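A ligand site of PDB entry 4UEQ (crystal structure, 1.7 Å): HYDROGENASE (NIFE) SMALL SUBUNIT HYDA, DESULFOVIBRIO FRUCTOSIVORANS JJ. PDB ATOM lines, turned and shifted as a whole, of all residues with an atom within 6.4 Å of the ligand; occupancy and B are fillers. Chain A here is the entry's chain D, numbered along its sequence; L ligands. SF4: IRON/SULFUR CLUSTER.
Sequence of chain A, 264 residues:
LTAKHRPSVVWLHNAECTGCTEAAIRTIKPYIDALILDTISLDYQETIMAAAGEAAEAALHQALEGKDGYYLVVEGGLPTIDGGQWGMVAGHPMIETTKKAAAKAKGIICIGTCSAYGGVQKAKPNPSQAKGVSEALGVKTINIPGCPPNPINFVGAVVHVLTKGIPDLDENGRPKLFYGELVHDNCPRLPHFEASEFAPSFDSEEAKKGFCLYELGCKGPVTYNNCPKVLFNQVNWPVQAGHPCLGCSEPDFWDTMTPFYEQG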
ATOM      1  N   VAL A 183      23.317  23.406  25.997  1.00  0.00           N
ATOM      2  CA  VAL A 183      24.088  22.786  27.096  1.00  0.00           C
ATOM      3  C   VAL A 183      25.164  21.838  26.536  1.00  0.00           C
ATOM      4  O   VAL A 183      26.355  21.916  26.885  1.00  0.00           O
ATOM      5  CB  VAL A 183      23.120  22.018  28.049  1.00  0.00           C
ATOM      6  CG1 VAL A 183      23.875  21.056  28.980  1.00  0.00           C
ATOM      7  CG2 VAL A 183      22.381  23.048  28.903  1.00  0.00           C
ATOM      8  N   HIS A 184      24.738  20.999  25.623  1.00  0.00           N
ATOM      9  CA  HIS A 184      25.566  19.945  25.030  1.00  0.00           C
ATOM     10  C   HIS A 184      26.803  20.516  24.319  1.00  0.00           C
ATOM     11  O   HIS A 184      27.872  19.908  24.350  1.00  0.00           O
ATOM     12  CB  HIS A 184      24.670  19.178  24.096  1.00  0.00           C
ATOM     13  CG  HIS A 184      25.356  18.178  23.217  1.00  0.00           C
ATOM     14  ND1 HIS A 184      25.716  16.915  23.667  1.00  0.00           N
ATOM     15  CD2 HIS A 184      25.618  18.191  21.892  1.00  0.00           C
ATOM     16  CE1 HIS A 184      26.207  16.217  22.654  1.00  0.00           C
ATOM     17  NE2 HIS A 184      26.137  16.966  21.564  1.00  0.00           N
ATOM     18  N   ASP A 185      26.674  21.688  23.693  1.00  0.00           N
ATOM     19  CA  ASP A 185      27.779  22.214  22.905  1.00  0.00           C
ATOM     20  C   ASP A 185      28.979  22.612  23.769  1.00  0.00           C
ATOM     21  O   ASP A 185      30.107  22.667  23.294  1.00  0.00           O
ATOM     22  CB  ASP A 185      27.306  23.362  21.984  1.00  0.00           C
ATOM     23  CG  ASP A 185      26.571  22.842  20.753  1.00  0.00           C
ATOM     24  OD1 ASP A 185      26.635  21.628  20.455  1.00  0.00           O
ATOM     25  OD2 ASP A 185      25.948  23.670  20.061  1.00  0.00           O
ATOM     26  N   CYS A 187      29.549  20.897  26.782  1.00  0.00           N
ATOM     27  CA  CYS A 187      29.684  19.853  27.800  1.00  0.00           C
ATOM     28  C   CYS A 187      31.055  19.209  27.715  1.00  0.00           C
ATOM     29  O   CYS A 187      31.479  18.807  26.626  1.00  0.00           O
ATOM     30  CB  CYS A 187      28.597  18.789  27.622  1.00  0.00           C
ATOM     31  SG  CYS A 187      28.739  17.469  28.862  1.00  0.00           S
ATOM     32  N   PRO A 188      31.745  19.046  28.873  1.00  0.00           N
ATOM     33  CA  PRO A 188      33.037  18.346  28.863  1.00  0.00           C
ATOM     34  C   PRO A 188      32.966  16.876  28.373  1.00  0.00           C
ATOM     35  O   PRO A 188      33.983  16.319  27.974  1.00  0.00           O
ATOM     36  CB  PRO A 188      33.473  18.417  30.331  1.00  0.00           C
ATOM     37  CG  PRO A 188      32.812  19.649  30.864  1.00  0.00           C
ATOM     38  CD  PRO A 188      31.490  19.750  30.154  1.00  0.00           C
ATOM     39  N   ARG A 189      31.790  16.266  28.402  1.00  0.00           N
ATOM     40  CA  ARG A 189      31.660  14.883  27.914  1.00  0.00           C
ATOM     41  C   ARG A 189      31.440  14.783  26.409  1.00  0.00           C
ATOM     42  O   ARG A 189      31.305  13.667  25.869  1.00  0.00           O
ATOM     43  CB  ARG A 189      30.568  14.137  28.689  1.00  0.00           C
ATOM     44  CG  ARG A 189      30.854  14.094  30.181  1.00  0.00           C
ATOM     45  CD  ARG A 189      29.934  13.160  30.936  1.00  0.00           C
ATOM     46  NE  ARG A 189      30.247  13.287  32.353  1.00  0.00           N
ATOM     47  CZ  ARG A 189      30.022  12.359  33.276  1.00  0.00           C
ATOM     48  NH1 ARG A 189      29.500  11.163  32.965  1.00  0.00           N
ATOM     49  NH2 ARG A 189      30.360  12.619  34.528  1.00  0.00           N
ATOM     50  N   LEU A 190      31.427  15.937  25.720  1.00  0.00           N
ATOM     51  CA  LEU A 190      31.179  15.978  24.266  1.00  0.00           C
ATOM     52  C   LEU A 190      32.105  15.055  23.463  1.00  0.00           C
ATOM     53  O   LEU A 190      31.623  14.367  22.556  1.00  0.00           O
ATOM     54  CB  LEU A 190      31.176  17.431  23.746  1.00  0.00           C
ATOM     55  CG  LEU A 190      30.872  17.643  22.262  1.00  0.00           C
ATOM     56  CD1 LEU A 190      29.443  17.234  21.916  1.00  0.00           C
ATOM     57  CD2 LEU A 190      31.120  19.113  21.897  1.00  0.00           C
ATOM     58  N   PRO A 191      33.422  14.997  23.802  1.00  0.00           N
ATOM     59  CA  PRO A 191      34.250  14.036  23.023  1.00  0.00           C
ATOM     60  C   PRO A 191      33.812  12.573  23.171  1.00  0.00           C
ATOM     61  O   PRO A 191      33.924  11.809  22.209  1.00  0.00           O
ATOM     62  CB  PRO A 191      35.680  14.245  23.538  1.00  0.00           C
ATOM     63  CG  PRO A 191      35.672  15.593  24.232  1.00  0.00           C
ATOM     64  CD  PRO A 191      34.253  15.827  24.703  1.00  0.00           C
ATOM     65  N   HIS A 192      33.273  12.199  24.349  1.00  0.00           N
ATOM     66  CA  HIS A 192      32.639  10.873  24.495  1.00  0.00           C
ATOM     67  C   HIS A 192      31.429  10.700  23.567  1.00  0.00           C
ATOM     68  O   HIS A 192      31.321   9.715  22.833  1.00  0.00           O
ATOM     69  CB  HIS A 192      32.249  10.581  25.949  1.00  0.00           C
ATOM     70  CG  HIS A 192      33.427  10.388  26.866  1.00  0.00           C
ATOM     71  ND1 HIS A 192      34.413   9.457  26.640  1.00  0.00           N
ATOM     72  CD2 HIS A 192      33.771  11.027  28.007  1.00  0.00           C
ATOM     73  CE1 HIS A 192      35.311   9.521  27.604  1.00  0.00           C
ATOM     74  NE2 HIS A 192      34.924  10.459  28.467  1.00  0.00           N
ATOM     75  N   PHE A 193      30.541  11.682  23.563  1.00  0.00           N
ATOM     76  CA  PHE A 193      29.372  11.677  22.652  1.00  0.00           C
ATOM     77  C   PHE A 193      29.853  11.482  21.219  1.00  0.00           C
ATOM     78  O   PHE A 193      29.316  10.645  20.492  1.00  0.00           O
ATOM     79  CB  PHE A 193      28.620  13.007  22.801  1.00  0.00           C
ATOM     80  CG  PHE A 193      27.384  13.146  21.932  1.00  0.00           C
ATOM     81  CD1 PHE A 193      27.476  13.705  20.644  1.00  0.00           C
ATOM     82  CD2 PHE A 193      26.120  12.750  22.424  1.00  0.00           C
ATOM     83  CE1 PHE A 193      26.351  13.888  19.879  1.00  0.00           C
ATOM     84  CE2 PHE A 193      24.977  12.929  21.616  1.00  0.00           C
ATOM     85  CZ  PHE A 193      25.108  13.493  20.344  1.00  0.00           C
ATOM     86  N   PHE A 198      29.071   5.804  25.454  1.00  0.00           N
ATOM     87  CA  PHE A 198      27.899   6.077  26.306  1.00  0.00           C
ATOM     88  C   PHE A 198      27.831   5.134  27.522  1.00  0.00           C
ATOM     89  O   PHE A 198      28.075   3.944  27.375  1.00  0.00           O
ATOM     90  CB  PHE A 198      26.623   5.895  25.495  1.00  0.00           C
ATOM     91  CG  PHE A 198      26.540   6.750  24.244  1.00  0.00           C
ATOM     92  CD1 PHE A 198      26.399   8.141  24.341  1.00  0.00           C
ATOM     93  CD2 PHE A 198      26.572   6.151  22.975  1.00  0.00           C
ATOM     94  CE1 PHE A 198      26.319   8.929  23.193  1.00  0.00           C
ATOM     95  CE2 PHE A 198      26.473   6.924  21.826  1.00  0.00           C
ATOM     96  CZ  PHE A 198      26.361   8.310  21.932  1.00  0.00           C
ATOM     97  N   PHE A 211      31.777   8.641  30.957  1.00  0.00           N
ATOM     98  CA  PHE A 211      31.213   8.576  29.608  1.00  0.00           C
ATOM     99  C   PHE A 211      29.921   9.427  29.500  1.00  0.00           C
ATOM    100  O   PHE A 211      29.292   9.806  30.522  1.00  0.00           O
ATOM    101  CB  PHE A 211      30.936   7.096  29.227  1.00  0.00           C
ATOM    102  CG  PHE A 211      32.139   6.335  28.754  1.00  0.00           C
ATOM    103  CD1 PHE A 211      33.437   6.744  29.092  1.00  0.00           C
ATOM    104  CD2 PHE A 211      31.978   5.228  27.936  1.00  0.00           C
ATOM    105  CE1 PHE A 211      34.545   6.029  28.611  1.00  0.00           C
ATOM    106  CE2 PHE A 211      33.056   4.497  27.482  1.00  0.00           C
ATOM    107  CZ  PHE A 211      34.356   4.898  27.800  1.00  0.00           C
ATOM    108  N   CYS A 212      29.562   9.750  28.258  1.00  0.00           N
ATOM    109  CA  CYS A 212      28.405  10.572  27.939  1.00  0.00           C
ATOM    110  C   CYS A 212      27.128   9.905  28.467  1.00  0.00           C
ATOM    111  O   CYS A 212      26.998   8.654  28.456  1.00  0.00           O
ATOM    112  CB  CYS A 212      28.321  10.833  26.395  1.00  0.00           C
ATOM    113  SG  CYS A 212      26.794  11.612  25.751  1.00  0.00           S
ATOM    114  N   LEU A 213      26.182  10.741  28.875  1.00  0.00           N
ATOM    115  CA  LEU A 213      24.927  10.273  29.519  1.00  0.00           C
ATOM    116  C   LEU A 213      23.712  10.255  28.571  1.00  0.00           C
ATOM    117  O   LEU A 213      22.565  10.104  29.027  1.00  0.00           O
ATOM    118  CB  LEU A 213      24.638  11.142  30.751  1.00  0.00           C
ATOM    119  CG  LEU A 213      25.785  11.192  31.786  1.00  0.00           C
ATOM    120  CD1 LEU A 213      25.469  12.196  32.884  1.00  0.00           C
ATOM    121  CD2 LEU A 213      26.089   9.809  32.385  1.00  0.00           C
ATOM    122  N   TYR A 214      23.954  10.358  27.249  1.00  0.00           N
ATOM    123  CA  TYR A 214      22.871  10.438  26.277  1.00  0.00           C
ATOM    124  C   TYR A 214      21.961   9.201  26.327  1.00  0.00           C
ATOM    125  O   TYR A 214      20.735   9.314  26.239  1.00  0.00           O
ATOM    126  CB  TYR A 214      23.438  10.565  24.853  1.00  0.00           C
ATOM    127  CG  TYR A 214      22.408  10.960  23.790  1.00  0.00           C
ATOM    128  CD1 TYR A 214      21.733  12.166  23.862  1.00  0.00           C
ATOM    129  CD2 TYR A 214      22.132  10.116  22.702  1.00  0.00           C
ATOM    130  CE1 TYR A 214      20.820  12.541  22.898  1.00  0.00           C
ATOM    131  CE2 TYR A 214      21.222  10.469  21.717  1.00  0.00           C
ATOM    132  CZ  TYR A 214      20.554  11.685  21.839  1.00  0.00           C
ATOM    133  OH  TYR A 214      19.647  12.090  20.888  1.00  0.00           O
ATOM    134  N   CYS A 218      20.044  11.990  28.787  1.00  0.00           N
ATOM    135  CA  CYS A 218      20.520  13.385  28.821  1.00  0.00           C
ATOM    136  C   CYS A 218      19.902  14.270  27.730  1.00  0.00           C
ATOM    137  O   CYS A 218      19.954  13.918  26.539  1.00  0.00           O
ATOM    138  CB  CYS A 218      22.039  13.446  28.729  1.00  0.00           C
ATOM    139  SG  CYS A 218      22.630  15.140  29.036  1.00  0.00           S
ATOM    140  N   LYS A 219      19.329  15.393  28.144  1.00  0.00           N
ATOM    141  CA  LYS A 219      18.600  16.300  27.202  1.00  0.00           C
ATOM    142  C   LYS A 219      19.456  17.469  26.803  1.00  0.00           C
ATOM    143  O   LYS A 219      18.998  18.422  26.152  1.00  0.00           O
ATOM    144  CB  LYS A 219      17.253  16.751  27.776  1.00  0.00           C
ATOM    145  CG  LYS A 219      16.268  15.622  28.066  1.00  0.00           C
ATOM    146  CD  LYS A 219      16.105  14.623  26.883  1.00  0.00           C
ATOM    147  CE  LYS A 219      15.012  13.561  27.187  1.00  0.00           C
ATOM    148  NZ  LYS A 219      15.180  12.816  28.495  1.00  0.00           N
ATOM    149  N   GLY A 220      20.737  17.371  27.135  1.00  0.00           N
ATOM    150  CA  GLY A 220      21.680  18.451  26.788  1.00  0.00           C
ATOM    151  C   GLY A 220      21.616  18.859  25.311  1.00  0.00           C
ATOM    152  O   GLY A 220      21.690  20.050  24.995  1.00  0.00           O
ATOM    153  N   PRO A 221      21.507  17.875  24.401  1.00  0.00           N
ATOM    154  CA  PRO A 221      21.511  18.206  22.959  1.00  0.00           C
ATOM    155  C   PRO A 221      20.294  19.016  22.467  1.00  0.00           C
ATOM    156  O   PRO A 221      20.336  19.497  21.327  1.00  0.00           O
ATOM    157  CB  PRO A 221      21.542  16.818  22.281  1.00  0.00           C
ATOM    158  CG  PRO A 221      22.144  15.923  23.308  1.00  0.00           C
ATOM    159  CD  PRO A 221      21.667  16.428  24.632  1.00  0.00           C
ATOM    160  N   TRP A 237      27.856  21.094  38.109  1.00  0.00           N
ATOM    161  CA  TRP A 237      26.597  21.086  37.377  1.00  0.00           C
ATOM    162  C   TRP A 237      26.175  19.628  37.214  1.00  0.00           C
ATOM    163  O   TRP A 237      26.979  18.746  37.465  1.00  0.00           O
ATOM    164  CB  TRP A 237      26.706  21.875  36.083  1.00  0.00           C
ATOM    165  CG  TRP A 237      27.481  21.195  34.980  1.00  0.00           C
ATOM    166  CD1 TRP A 237      28.853  21.007  34.923  1.00  0.00           C
ATOM    167  CD2 TRP A 237      26.957  20.690  33.740  1.00  0.00           C
ATOM    168  NE1 TRP A 237      29.186  20.365  33.751  1.00  0.00           N
ATOM    169  CE2 TRP A 237      28.047  20.184  33.003  1.00  0.00           C
ATOM    170  CE3 TRP A 237      25.656  20.620  33.185  1.00  0.00           C
ATOM    171  CZ2 TRP A 237      27.887  19.594  31.723  1.00  0.00           C
ATOM    172  CZ3 TRP A 237      25.495  20.030  31.904  1.00  0.00           C
ATOM    173  CH2 TRP A 237      26.612  19.536  31.205  1.00  0.00           C
ATOM    174  N   VAL A 239      25.653  17.203  35.021  1.00  0.00           N
ATOM    175  CA  VAL A 239      26.405  16.185  34.259  1.00  0.00           C
ATOM    176  C   VAL A 239      27.763  15.951  34.926  1.00  0.00           C
ATOM    177  O   VAL A 239      28.240  14.829  34.982  1.00  0.00           O
ATOM    178  CB  VAL A 239      26.529  16.554  32.753  1.00  0.00           C
ATOM    179  CG1 VAL A 239      27.536  15.665  32.059  1.00  0.00           C
ATOM    180  CG2 VAL A 239      25.157  16.451  32.060  1.00  0.00           C
ATOM    181  N   PRO A 244      22.144  12.897  33.968  1.00  0.00           N
ATOM    182  CA  PRO A 244      21.678  13.558  32.744  1.00  0.00           C
ATOM    183  C   PRO A 244      20.970  14.889  33.016  1.00  0.00           C
ATOM    184  O   PRO A 244      20.388  15.075  34.089  1.00  0.00           O
ATOM    185  CB  PRO A 244      20.723  12.526  32.126  1.00  0.00           C
ATOM    186  CG  PRO A 244      20.270  11.706  33.323  1.00  0.00           C
ATOM    187  CD  PRO A 244      21.494  11.600  34.169  1.00  0.00           C
ATOM    188  N   CYS A 245      21.057  15.801  32.057  1.00  0.00           N
ATOM    189  CA  CYS A 245      20.276  17.028  32.016  1.00  0.00           C
ATOM    190  C   CYS A 245      18.797  16.654  31.787  1.00  0.00           C
ATOM    191  O   CYS A 245      18.493  15.733  31.011  1.00  0.00           O
ATOM    192  CB  CYS A 245      20.816  17.931  30.892  1.00  0.00           C
ATOM    193  SG  CYS A 245      19.834  19.411  30.549  1.00  0.00           S
ATOM    194  N   GLN A 263      15.469   8.472  25.834  1.00  0.00           N
ATOM    195  CA  GLN A 263      15.277   9.435  24.716  1.00  0.00           C
ATOM    196  C   GLN A 263      13.934   9.283  23.963  1.00  0.00           C
ATOM    197  O   GLN A 263      13.605  10.098  23.082  1.00  0.00           O
ATOM    198  CB  GLN A 263      16.437   9.367  23.701  1.00  0.00           C
ATOM    199  CG  GLN A 263      17.839   9.771  24.180  1.00  0.00           C
ATOM    200  CD  GLN A 263      17.940  11.197  24.751  1.00  0.00           C
ATOM    201  OE1 GLN A 263      17.154  12.056  24.395  1.00  0.00           O
ATOM    202  NE2 GLN A 263      18.927  11.430  25.594  1.00  0.00           N
HETATM  203 FE1  SF4 L   1      24.624  15.180  27.839  1.00  0.00          FE
HETATM  204 FE2  SF4 L   1      26.593  13.671  26.582  1.00  0.00          FE
HETATM  205 FE3  SF4 L   1      27.196  16.020  27.812  1.00  0.00          FE
HETATM  206 FE4  SF4 L   1      25.787  16.032  25.548  1.00  0.00          FE
HETATM  207  S1  SF4 L   1      27.952  15.253  25.754  1.00  0.00           S
HETATM  208  S2  SF4 L   1      25.336  17.303  27.311  1.00  0.00           S
HETATM  209  S3  SF4 L   1      24.478  14.158  25.829  1.00  0.00           S
HETATM  210  S4  SF4 L   1      26.461  14.147  28.834  1.00  0.00           S
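N of Tyr 214 lies close to SG of Cys 212 (3.4 Å). The backbone NH (N) of Cys 245 lies close to the side-chain sulfur (SG) of Cys 218, at 3.5 Å. The side-chain sulfur of Cys 187 lies close to the backbone NH of Arg 189. N of His 184 sits close to O of Gly 220 (3.3 Å). The guanidinium group (NH1) of Arg 189 lies within hydrogen-bond range of the backbone carbonyl oxygen (O) of Phe 211 (2.8 Å). NH2 of Arg 189 sits at hydrogen-bond distance from O of Val 239. The side-chain amide nitrogen (NE2) of Gln 263 is in hydrogen-bond range of the backbone carbonyl oxygen (O) of Tyr 214 (2.9 Å). The backbone NH (N) of Gly 220 sits close to the side-chain sulfur (SG) of Cys 218, 3.5 Å away.
The side-chain sulfur (SG) of Cys 218 is bound to an iron atom (FE1) of the ligand (2.3 Å). The side-chain sulfur (SG) of Cys 212 is bound to an iron atom (FE2) of the ligand (2.2 Å). The backbone NH (N) of Leu 190 sits close to a sulfur (S1) of the ligand (3.5 Å). An iron atom (FE3) of the ligand is bound by the side-chain sulfur (SG) of Cys 187 (2.4 Å). The backbone NH (N) of Leu 213 sits close to a sulfur (S4) of the ligand, at 3.4 Å. A ring nitrogen (ND1) of His 184 is bound to an iron atom (FE4) of the ligand (2.1 Å).
A sulfur (S1) of the ligand lies close to the backbone carbonyl oxygen (O) of Arg 189 (3.7 Å). Merely in contact with the ligand: Phe 193 (3.8 Å), Tyr 214 (3.9 Å), Gly 220 (3.9 Å), Pro 221 (3.8 Å) and Val 239 (3.7 Å). Hydrophobic or aromatic side chains within 4 Å of the ligand: His 184, Phe 193, Tyr 214, Pro 221 and Val 239. The nearest printed residue that does not touch the ligand is Val 183 (4.4 Å).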
